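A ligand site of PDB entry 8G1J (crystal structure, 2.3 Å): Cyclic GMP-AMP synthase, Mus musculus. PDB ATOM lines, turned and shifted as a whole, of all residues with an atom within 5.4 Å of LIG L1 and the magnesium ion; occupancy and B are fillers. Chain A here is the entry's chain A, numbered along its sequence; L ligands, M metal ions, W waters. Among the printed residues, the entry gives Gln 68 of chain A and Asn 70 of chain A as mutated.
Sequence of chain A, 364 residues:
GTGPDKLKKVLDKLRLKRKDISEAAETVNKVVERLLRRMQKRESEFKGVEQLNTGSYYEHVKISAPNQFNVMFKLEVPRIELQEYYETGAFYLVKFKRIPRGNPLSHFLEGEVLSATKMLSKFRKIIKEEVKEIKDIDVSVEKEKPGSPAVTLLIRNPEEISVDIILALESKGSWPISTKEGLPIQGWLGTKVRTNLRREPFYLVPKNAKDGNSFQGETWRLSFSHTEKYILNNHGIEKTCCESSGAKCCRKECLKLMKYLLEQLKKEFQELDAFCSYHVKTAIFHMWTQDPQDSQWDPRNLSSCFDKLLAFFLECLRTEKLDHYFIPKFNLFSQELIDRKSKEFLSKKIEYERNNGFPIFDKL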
ATOM      1  N   THR A  54      16.634  -8.460  22.168  1.00  0.00           N
ATOM      2  CA  THR A  54      17.287  -9.782  22.305  1.00  0.00           C
ATOM      3  C   THR A  54      17.045 -10.621  21.056  1.00  0.00           C
ATOM      4  O   THR A  54      16.314 -10.224  20.136  1.00  0.00           O
ATOM      5  CB  THR A  54      16.762 -10.548  23.514  1.00  0.00           C
ATOM      6  OG1 THR A  54      15.346 -10.699  23.375  1.00  0.00           O
ATOM      7  CG2 THR A  54      17.027  -9.814  24.784  1.00  0.00           C
ATOM      8  N   GLY A  55      17.637 -11.810  21.032  1.00  0.00           N
ATOM      9  CA  GLY A  55      17.313 -12.725  19.959  1.00  0.00           C
ATOM     10  C   GLY A  55      18.090 -12.451  18.687  1.00  0.00           C
ATOM     11  O   GLY A  55      18.946 -11.556  18.621  1.00  0.00           O
ATOM     12  N   SER A  56      17.767 -13.233  17.650  1.00  0.00           N
ATOM     13  CA  SER A  56      18.681 -13.403  16.518  1.00  0.00           C
ATOM     14  C   SER A  56      18.911 -12.110  15.758  1.00  0.00           C
ATOM     15  O   SER A  56      20.017 -11.896  15.242  1.00  0.00           O
ATOM     16  CB  SER A  56      18.157 -14.471  15.536  1.00  0.00           C
ATOM     17  OG  SER A  56      16.920 -14.099  14.938  1.00  0.00           O
ATOM     18  N   GLN A  68      11.080 -11.197  12.269  1.00  0.00           N
ATOM     19  CA  GLN A  68      10.795 -11.672  13.626  1.00  0.00           C
ATOM     20  C   GLN A  68      11.755 -10.989  14.573  1.00  0.00           C
ATOM     21  O   GLN A  68      12.959 -11.235  14.491  1.00  0.00           O
ATOM     22  CB  GLN A  68      10.902 -13.200  13.741  1.00  0.00           C
ATOM     23  CG  GLN A  68      10.048 -13.757  14.872  1.00  0.00           C
ATOM     24  CD  GLN A  68      10.825 -14.036  16.143  1.00  0.00           C
ATOM     25  OE1 GLN A  68      12.005 -13.665  16.282  1.00  0.00           O
ATOM     26  NE2 GLN A  68      10.177 -14.711  17.090  1.00  0.00           N
ATOM     27  N   PHE A  69      11.236 -10.126  15.455  1.00  0.00           N
ATOM     28  CA  PHE A  69      12.014  -9.361  16.423  1.00  0.00           C
ATOM     29  C   PHE A  69      11.624  -9.780  17.841  1.00  0.00           C
ATOM     30  O   PHE A  69      10.459 -10.069  18.120  1.00  0.00           O
ATOM     31  CB  PHE A  69      11.789  -7.829  16.277  1.00  0.00           C
ATOM     32  CG  PHE A  69      12.198  -7.263  14.919  1.00  0.00           C
ATOM     33  CD1 PHE A  69      11.476  -7.569  13.766  1.00  0.00           C
ATOM     34  CD2 PHE A  69      13.299  -6.414  14.804  1.00  0.00           C
ATOM     35  CE1 PHE A  69      11.860  -7.050  12.534  1.00  0.00           C
ATOM     36  CE2 PHE A  69      13.683  -5.894  13.572  1.00  0.00           C
ATOM     37  CZ  PHE A  69      12.940  -6.218  12.437  1.00  0.00           C
ATOM     38  N   ASN A  70      12.614  -9.815  18.721  1.00  0.00           N
ATOM     39  CA  ASN A  70      12.412 -10.221  20.112  1.00  0.00           C
ATOM     40  C   ASN A  70      12.787  -9.063  21.022  1.00  0.00           C
ATOM     41  O   ASN A  70      13.903  -8.534  20.925  1.00  0.00           O
ATOM     42  CB  ASN A  70      13.253 -11.446  20.455  1.00  0.00           C
ATOM     43  CG  ASN A  70      12.972 -12.616  19.532  1.00  0.00           C
ATOM     44  OD1 ASN A  70      13.751 -12.898  18.619  1.00  0.00           O
ATOM     45  ND2 ASN A  70      11.834 -13.298  19.753  1.00  0.00           N
ATOM     46  N   MET A  72      12.383  -7.657  25.158  1.00  0.00           N
ATOM     47  CA  MET A  72      11.968  -7.918  26.530  1.00  0.00           C
ATOM     48  C   MET A  72      11.612  -6.591  27.189  1.00  0.00           C
ATOM     49  O   MET A  72      12.364  -5.612  27.092  1.00  0.00           O
ATOM     50  CB  MET A  72      13.063  -8.609  27.356  1.00  0.00           C
ATOM     51  CG  MET A  72      13.854  -9.679  26.641  1.00  0.00           C
ATOM     52  SD  MET A  72      14.480 -11.039  27.676  1.00  0.00           S
ATOM     53  CE  MET A  72      14.740 -10.226  29.262  1.00  0.00           C
ATOM     54  N   LYS A 145      -1.024 -18.014  22.703  1.00  0.00           N
ATOM     55  CA  LYS A 145      -0.662 -19.438  22.797  1.00  0.00           C
ATOM     56  C   LYS A 145      -0.584 -19.830  24.266  1.00  0.00           C
ATOM     57  O   LYS A 145       0.196 -19.208  25.013  1.00  0.00           O
ATOM     58  CB  LYS A 145       0.676 -19.728  22.147  1.00  0.00           C
ATOM     59  CG  LYS A 145       0.979 -18.944  20.888  1.00  0.00           C
ATOM     60  CD  LYS A 145       0.499 -19.663  19.642  1.00  0.00           C
ATOM     61  CE  LYS A 145       0.459 -18.695  18.460  1.00  0.00           C
ATOM     62  NZ  LYS A 145      -0.883 -18.698  17.785  1.00  0.00           N
ATOM     63  N   PRO A 146      -1.334 -20.826  24.728  1.00  0.00           N
ATOM     64  CA  PRO A 146      -1.293 -21.177  26.162  1.00  0.00           C
ATOM     65  C   PRO A 146       0.118 -21.544  26.601  1.00  0.00           C
ATOM     66  O   PRO A 146       0.872 -22.189  25.871  1.00  0.00           O
ATOM     67  CB  PRO A 146      -2.251 -22.367  26.253  1.00  0.00           C
ATOM     68  CG  PRO A 146      -3.195 -22.196  25.097  1.00  0.00           C
ATOM     69  CD  PRO A 146      -2.393 -21.553  23.996  1.00  0.00           C
ATOM     70  N   GLY A 147       0.475 -21.090  27.810  1.00  0.00           N
ATOM     71  CA  GLY A 147       1.795 -21.303  28.389  1.00  0.00           C
ATOM     72  C   GLY A 147       2.943 -20.531  27.765  1.00  0.00           C
ATOM     73  O   GLY A 147       4.103 -20.801  28.100  1.00  0.00           O
ATOM     74  N   SER A 148       2.667 -19.595  26.860  1.00  0.00           N
ATOM     75  CA  SER A 148       3.691 -18.782  26.196  1.00  0.00           C
ATOM     76  C   SER A 148       3.941 -17.484  26.961  1.00  0.00           C
ATOM     77  O   SER A 148       2.996 -16.839  27.420  1.00  0.00           O
ATOM     78  CB  SER A 148       3.281 -18.459  24.773  1.00  0.00           C
ATOM     79  OG  SER A 148       4.317 -17.772  24.101  1.00  0.00           O
ATOM     80  N   PRO A 149       5.182 -17.059  27.127  1.00  0.00           N
ATOM     81  CA  PRO A 149       5.442 -15.799  27.831  1.00  0.00           C
ATOM     82  C   PRO A 149       5.199 -14.565  26.973  1.00  0.00           C
ATOM     83  O   PRO A 149       5.329 -13.440  27.488  1.00  0.00           O
ATOM     84  CB  PRO A 149       6.926 -15.899  28.205  1.00  0.00           C
ATOM     85  CG  PRO A 149       7.495 -16.721  27.071  1.00  0.00           C
ATOM     86  CD  PRO A 149       6.433 -17.720  26.697  1.00  0.00           C
ATOM     87  N   ALA A 150       4.871 -14.727  25.695  1.00  0.00           N
ATOM     88  CA  ALA A 150       4.978 -13.632  24.754  1.00  0.00           C
ATOM     89  C   ALA A 150       3.633 -12.991  24.451  1.00  0.00           C
ATOM     90  O   ALA A 150       2.574 -13.631  24.475  1.00  0.00           O
ATOM     91  CB  ALA A 150       5.610 -14.109  23.445  1.00  0.00           C
ATOM     92  N   ASP A 164       7.720 -10.434  19.201  1.00  0.00           N
ATOM     93  CA  ASP A 164       7.435 -11.097  20.469  1.00  0.00           C
ATOM     94  C   ASP A 164       7.855 -10.138  21.565  1.00  0.00           C
ATOM     95  O   ASP A 164       9.038  -9.839  21.717  1.00  0.00           O
ATOM     96  CB  ASP A 164       8.189 -12.421  20.572  1.00  0.00           C
ATOM     97  CG  ASP A 164       7.546 -13.546  19.757  1.00  0.00           C
ATOM     98  OD1 ASP A 164       6.499 -13.304  19.131  1.00  0.00           O
ATOM     99  OD2 ASP A 164       8.077 -14.678  19.770  1.00  0.00           O
ATOM    100  N   ILE A 166       8.106  -9.700  25.438  1.00  0.00           N
ATOM    101  CA  ILE A 166       8.266 -10.665  26.520  1.00  0.00           C
ATOM    102  C   ILE A 166       8.372  -9.884  27.818  1.00  0.00           C
ATOM    103  O   ILE A 166       9.349  -9.154  28.044  1.00  0.00           O
ATOM    104  CB  ILE A 166       9.510 -11.546  26.296  1.00  0.00           C
ATOM    105  CG1 ILE A 166       9.235 -12.569  25.196  1.00  0.00           C
ATOM    106  CG2 ILE A 166       9.886 -12.254  27.558  1.00  0.00           C
ATOM    107  N   VAL A 205      10.612 -15.134  33.051  1.00  0.00           N
ATOM    108  CA  VAL A 205       9.528 -14.890  32.117  1.00  0.00           C
ATOM    109  C   VAL A 205       8.403 -15.868  32.424  1.00  0.00           C
ATOM    110  O   VAL A 205       8.664 -16.966  32.951  1.00  0.00           O
ATOM    111  CB  VAL A 205      10.010 -15.016  30.669  1.00  0.00           C
ATOM    112  CG1 VAL A 205      11.228 -14.123  30.481  1.00  0.00           C
ATOM    113  CG2 VAL A 205      10.322 -16.474  30.322  1.00  0.00           C
ATOM    114  N   ARG A 221       9.939 -18.843  34.336  1.00  0.00           N
ATOM    115  CA  ARG A 221      11.067 -19.531  33.711  1.00  0.00           C
ATOM    116  C   ARG A 221      12.263 -18.588  33.593  1.00  0.00           C
ATOM    117  O   ARG A 221      12.104 -17.424  33.188  1.00  0.00           O
ATOM    118  CB  ARG A 221      10.719 -20.078  32.287  1.00  0.00           C
ATOM    119  CG  ARG A 221      11.906 -20.851  31.639  1.00  0.00           C
ATOM    120  CD  ARG A 221      11.584 -21.449  30.271  1.00  0.00           C
ATOM    121  NE  ARG A 221      11.481 -20.405  29.259  1.00  0.00           N
ATOM    122  CZ  ARG A 221      11.043 -20.600  28.010  1.00  0.00           C
ATOM    123  NH1 ARG A 221      10.654 -21.798  27.596  1.00  0.00           N
ATOM    124  NH2 ARG A 221      10.990 -19.570  27.177  1.00  0.00           N
ATOM    125  N   LEU A 222      13.451 -19.103  33.908  1.00  0.00           N
ATOM    126  CA  LEU A 222      14.666 -18.299  33.789  1.00  0.00           C
ATOM    127  C   LEU A 222      14.942 -17.932  32.337  1.00  0.00           C
ATOM    128  O   LEU A 222      14.732 -18.740  31.428  1.00  0.00           O
ATOM    129  CB  LEU A 222      15.878 -19.040  34.336  1.00  0.00           C
ATOM    130  CG  LEU A 222      15.955 -19.108  35.840  1.00  0.00           C
ATOM    131  CD1 LEU A 222      17.023 -20.108  36.237  1.00  0.00           C
ATOM    132  CD2 LEU A 222      16.264 -17.711  36.371  1.00  0.00           C
ATOM    133  N   SER A 223      15.440 -16.719  32.123  1.00  0.00           N
ATOM    134  CA  SER A 223      15.876 -16.261  30.809  1.00  0.00           C
ATOM    135  C   SER A 223      17.275 -15.688  30.879  1.00  0.00           C
ATOM    136  O   SER A 223      17.576 -14.869  31.764  1.00  0.00           O
ATOM    137  CB  SER A 223      14.946 -15.201  30.244  1.00  0.00           C
ATOM    138  OG  SER A 223      15.456 -14.719  29.011  1.00  0.00           O
ATOM    139  N   PHE A 224      18.117 -16.060  29.915  1.00  0.00           N
ATOM    140  CA  PHE A 224      19.472 -15.537  29.813  1.00  0.00           C
ATOM    141  C   PHE A 224      19.721 -14.866  28.470  1.00  0.00           C
ATOM    142  O   PHE A 224      20.846 -14.893  27.956  1.00  0.00           O
ATOM    143  CB  PHE A 224      20.476 -16.669  30.056  1.00  0.00           C
ATOM    144  CG  PHE A 224      20.352 -17.264  31.397  1.00  0.00           C
ATOM    145  CD1 PHE A 224      20.917 -16.655  32.481  1.00  0.00           C
ATOM    146  CD2 PHE A 224      19.558 -18.389  31.584  1.00  0.00           C
ATOM    147  CE1 PHE A 224      20.768 -17.182  33.725  1.00  0.00           C
ATOM    148  CE2 PHE A 224      19.388 -18.919  32.846  1.00  0.00           C
ATOM    149  CZ  PHE A 224      20.016 -18.317  33.916  1.00  0.00           C
ATOM    150  N   SER A 225      18.683 -14.257  27.897  1.00  0.00           N
ATOM    151  CA  SER A 225      18.798 -13.692  26.564  1.00  0.00           C
ATOM    152  C   SER A 225      19.857 -12.608  26.507  1.00  0.00           C
ATOM    153  O   SER A 225      20.515 -12.453  25.482  1.00  0.00           O
ATOM    154  CB  SER A 225      17.460 -13.118  26.114  1.00  0.00           C
ATOM    155  OG  SER A 225      16.537 -14.166  26.029  1.00  0.00           O
HETATM  156  P1  LIG L   1       7.332 -24.267  23.878  1.00  0.00           P
HETATM  157  O1  LIG L   1       7.919 -23.668  22.592  1.00  0.00           O
HETATM  158  O2  LIG L   1       8.398 -24.894  24.768  1.00  0.00           O
HETATM  159  O3  LIG L   1       6.282 -25.285  23.482  1.00  0.00           O
HETATM  160  O4  LIG L   1       6.622 -23.145  24.786  1.00  0.00           O
HETATM  161  P2  LIG L   1       5.996 -21.777  24.183  1.00  0.00           P
HETATM  162  O5  LIG L   1       5.866 -21.835  22.672  1.00  0.00           O
HETATM  163  O6  LIG L   1       4.694 -21.444  24.881  1.00  0.00           O
HETATM  164  O7  LIG L   1       7.160 -20.751  24.626  1.00  0.00           O
HETATM  165  P3  LIG L   1       8.532 -20.516  23.822  1.00  0.00           P
HETATM  166  O8  LIG L   1       9.661 -21.043  24.683  1.00  0.00           O
HETATM  167  O9  LIG L   1       8.535 -21.074  22.416  1.00  0.00           O
HETATM  168  O10 LIG L   1       8.533 -18.905  23.772  1.00  0.00           O
HETATM  169  C1  LIG L   1       7.657 -18.253  22.879  1.00  0.00           C
HETATM  170  C2  LIG L   1       8.416 -17.128  22.186  1.00  0.00           C
HETATM  171  O11 LIG L   1       8.602 -16.090  23.139  1.00  0.00           O
HETATM  172  C3  LIG L   1       9.818 -17.516  21.718  1.00  0.00           C
HETATM  173  O12 LIG L   1       9.843 -18.035  20.410  1.00  0.00           O
HETATM  174  C4  LIG L   1      10.534 -16.182  21.816  1.00  0.00           C
HETATM  175  O13 LIG L   1      10.248 -15.430  20.647  1.00  0.00           O
HETATM  176  C5  LIG L   1       9.898 -15.514  23.021  1.00  0.00           C
HETATM  177  N1  LIG L   1      10.714 -15.848  24.207  1.00  0.00           N
HETATM  178  C6  LIG L   1      10.540 -16.962  25.010  1.00  0.00           C
HETATM  179  N2  LIG L   1      11.468 -16.925  26.006  1.00  0.00           N
HETATM  180  C7  LIG L   1      12.225 -15.807  25.863  1.00  0.00           C
HETATM  181  C8  LIG L   1      13.323 -15.303  26.579  1.00  0.00           C
HETATM  182  O14 LIG L   1      13.752 -15.895  27.559  1.00  0.00           O
HETATM  183  N3  LIG L   1      13.913 -14.113  26.183  1.00  0.00           N
HETATM  184  C9  LIG L   1      13.454 -13.444  25.070  1.00  0.00           C
HETATM  185  N4  LIG L   1      12.375 -13.961  24.352  1.00  0.00           N
HETATM  186  C10 LIG L   1      11.769 -15.123  24.734  1.00  0.00           C
HETATM  187  P1  LG2 L   2      14.928 -16.924  15.386  1.00  0.00           P
HETATM  188  O1  LG2 L   2      14.343 -18.277  15.230  1.00  0.00           O
HETATM  189  O2  LG2 L   2      15.742 -16.430  14.185  1.00  0.00           O
HETATM  190  O3  LG2 L   2      13.900 -15.862  15.765  1.00  0.00           O
HETATM  191  P2  LG2 L   2      15.948 -16.428  18.128  1.00  0.00           P
HETATM  192  O4  LG2 L   2      17.196 -16.773  18.886  1.00  0.00           O
HETATM  193  O5  LG2 L   2      15.581 -14.939  18.128  1.00  0.00           O
HETATM  194  O6  LG2 L   2      15.942 -16.916  16.623  1.00  0.00           O
HETATM  195  P3  LG2 L   2      13.278 -16.885  19.308  1.00  0.00           P
HETATM  196  O7  LG2 L   2      12.427 -18.099  19.257  1.00  0.00           O
HETATM  197  O8  LG2 L   2      12.784 -15.674  18.557  1.00  0.00           O
HETATM  198  O9  LG2 L   2      14.699 -17.234  18.693  1.00  0.00           O
HETATM  199  O10 LG2 L   2      13.563 -16.615  20.842  1.00  0.00           O
HETATM  200  C1  LG2 L   2      14.180 -15.392  21.299  1.00  0.00           C
HETATM  201  C2  LG2 L   2      15.132 -15.661  22.449  1.00  0.00           C
HETATM  202  O11 LG2 L   2      14.414 -16.164  23.596  1.00  0.00           O
HETATM  203  C3  LG2 L   2      16.226 -16.697  22.197  1.00  0.00           C
HETATM  204  O12 LG2 L   2      17.336 -16.124  21.516  1.00  0.00           O
HETATM  205  C4  LG2 L   2      16.558 -17.183  23.610  1.00  0.00           C
HETATM  206  O13 LG2 L   2      17.472 -16.354  24.319  1.00  0.00           O
HETATM  207  C5  LG2 L   2      15.194 -17.105  24.312  1.00  0.00           C
HETATM  208  N1  LG2 L   2      14.486 -18.380  24.311  1.00  0.00           N
HETATM  209  C6  LG2 L   2      13.701 -18.886  23.293  1.00  0.00           C
HETATM  210  N2  LG2 L   2      13.211 -20.080  23.552  1.00  0.00           N
HETATM  211  C7  LG2 L   2      13.738 -20.394  24.786  1.00  0.00           C
HETATM  212  C8  LG2 L   2      13.603 -21.527  25.621  1.00  0.00           C
HETATM  213  N3  LG2 L   2      12.862 -22.600  25.306  1.00  0.00           N
HETATM  214  N4  LG2 L   2      14.246 -21.515  26.805  1.00  0.00           N
HETATM  215  C9  LG2 L   2      14.979 -20.451  27.141  1.00  0.00           C
HETATM  216  N5  LG2 L   2      15.183 -19.333  26.430  1.00  0.00           N
HETATM  217  C10 LG2 L   2      14.527 -19.363  25.271  1.00  0.00           C
HETATM  218 MG    MG M   1      13.742 -14.462  17.133  1.00  0.00          MG
HETATM  219  O   HOH W   1      14.662 -12.819  15.905  1.00  0.00           O
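An oxygen (O13) of LIG L1 sits at hydrogen-bond distance from the side-chain amide nitrogen (ND2) of Asn 70 (2.8 Å).
OD2 of Asp 164 lies within hydrogen-bond range of O13 of LIG L1 (2.5 Å).
The side-chain hydroxyl of Ser 223 sits at hydrogen-bond distance from an oxygen (O14) of LIG L1 (2.5 Å).
The side-chain hydroxyl of Ser 225 is in hydrogen-bond range of a nitrogen (N3) of LIG L1.
O8 of LIG L1 is in salt-bridge range of NH1 of Arg 221 (3.2 Å).
O6 of LIG L1 sits close to N of Ser 148, at 3.4 Å.
A nitrogen (N3) of LIG L1 sits at hydrogen-bond distance from the side-chain sulfur of Met 72, at 3.5 Å.
OG of Ser 225 lies within hydrogen-bond range of O13 of LG2 L2.
O5 of LG2 L2 lies close to N of Ser 56, at 2.8 Å.
The side-chain hydroxyl of Ser 56 sits at hydrogen-bond distance from an oxygen (O2) of LG2 L2, 2.7 Å away.
An oxygen (O12) of LIG L1 lies within hydrogen-bond range of an oxygen (O7) of LG2 L2 (2.8 Å).
OD2 of Asp 164 is in hydrogen-bond range of NE2 of Gln 68 (3.4 Å).
O of Asn 70 is in hydrogen-bond range of N of Thr 54.
The backbone NH (N) of Asp 164 sits at hydrogen-bond distance from the backbone carbonyl oxygen (O) of Phe 69 (3.0 Å).
The side-chain hydroxyl (OG) of Ser 223 lies within hydrogen-bond range of the side-chain hydroxyl (OG) of Ser 225 (3.2 Å).
The backbone NH (N) of Arg 221 is in hydrogen-bond range of the backbone carbonyl oxygen (O) of Val 205, 2.7 Å away.
The side-chain hydroxyl of Ser 148 lies close to the backbone NH of Ala 150 (3.5 Å).
O6 of LIG L1 lies close to O of Gly 147, 3.3 Å away.
Residues that only touch LIG L1: Thr 54, Pro 149, Ala 150 and Ile 166.
OG of Ser 56 touches the magnesium ion, 3.9 Å away.
Along chain A the residues within 4 Å of the magnesium ion span positions 56 to 70.
The magnesium ion is bound by O3 of LG2 L2 (2.0 Å), OE1 of Gln 68 (2.1 Å), O8 of LG2 L2 (2.1 Å), O5 of LG2 L2 (2.1 Å), OD1 of Asn 70 (2.2 Å) and water W1 (2.2 Å).
The magnesium ion has six donor atoms within binding distance.
Water W1 bridges the backbone carbonyl oxygen (O) of Gln 68 (2.7 Å) and the side-chain hydroxyl (OG) of Ser 56 (2.8 Å).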
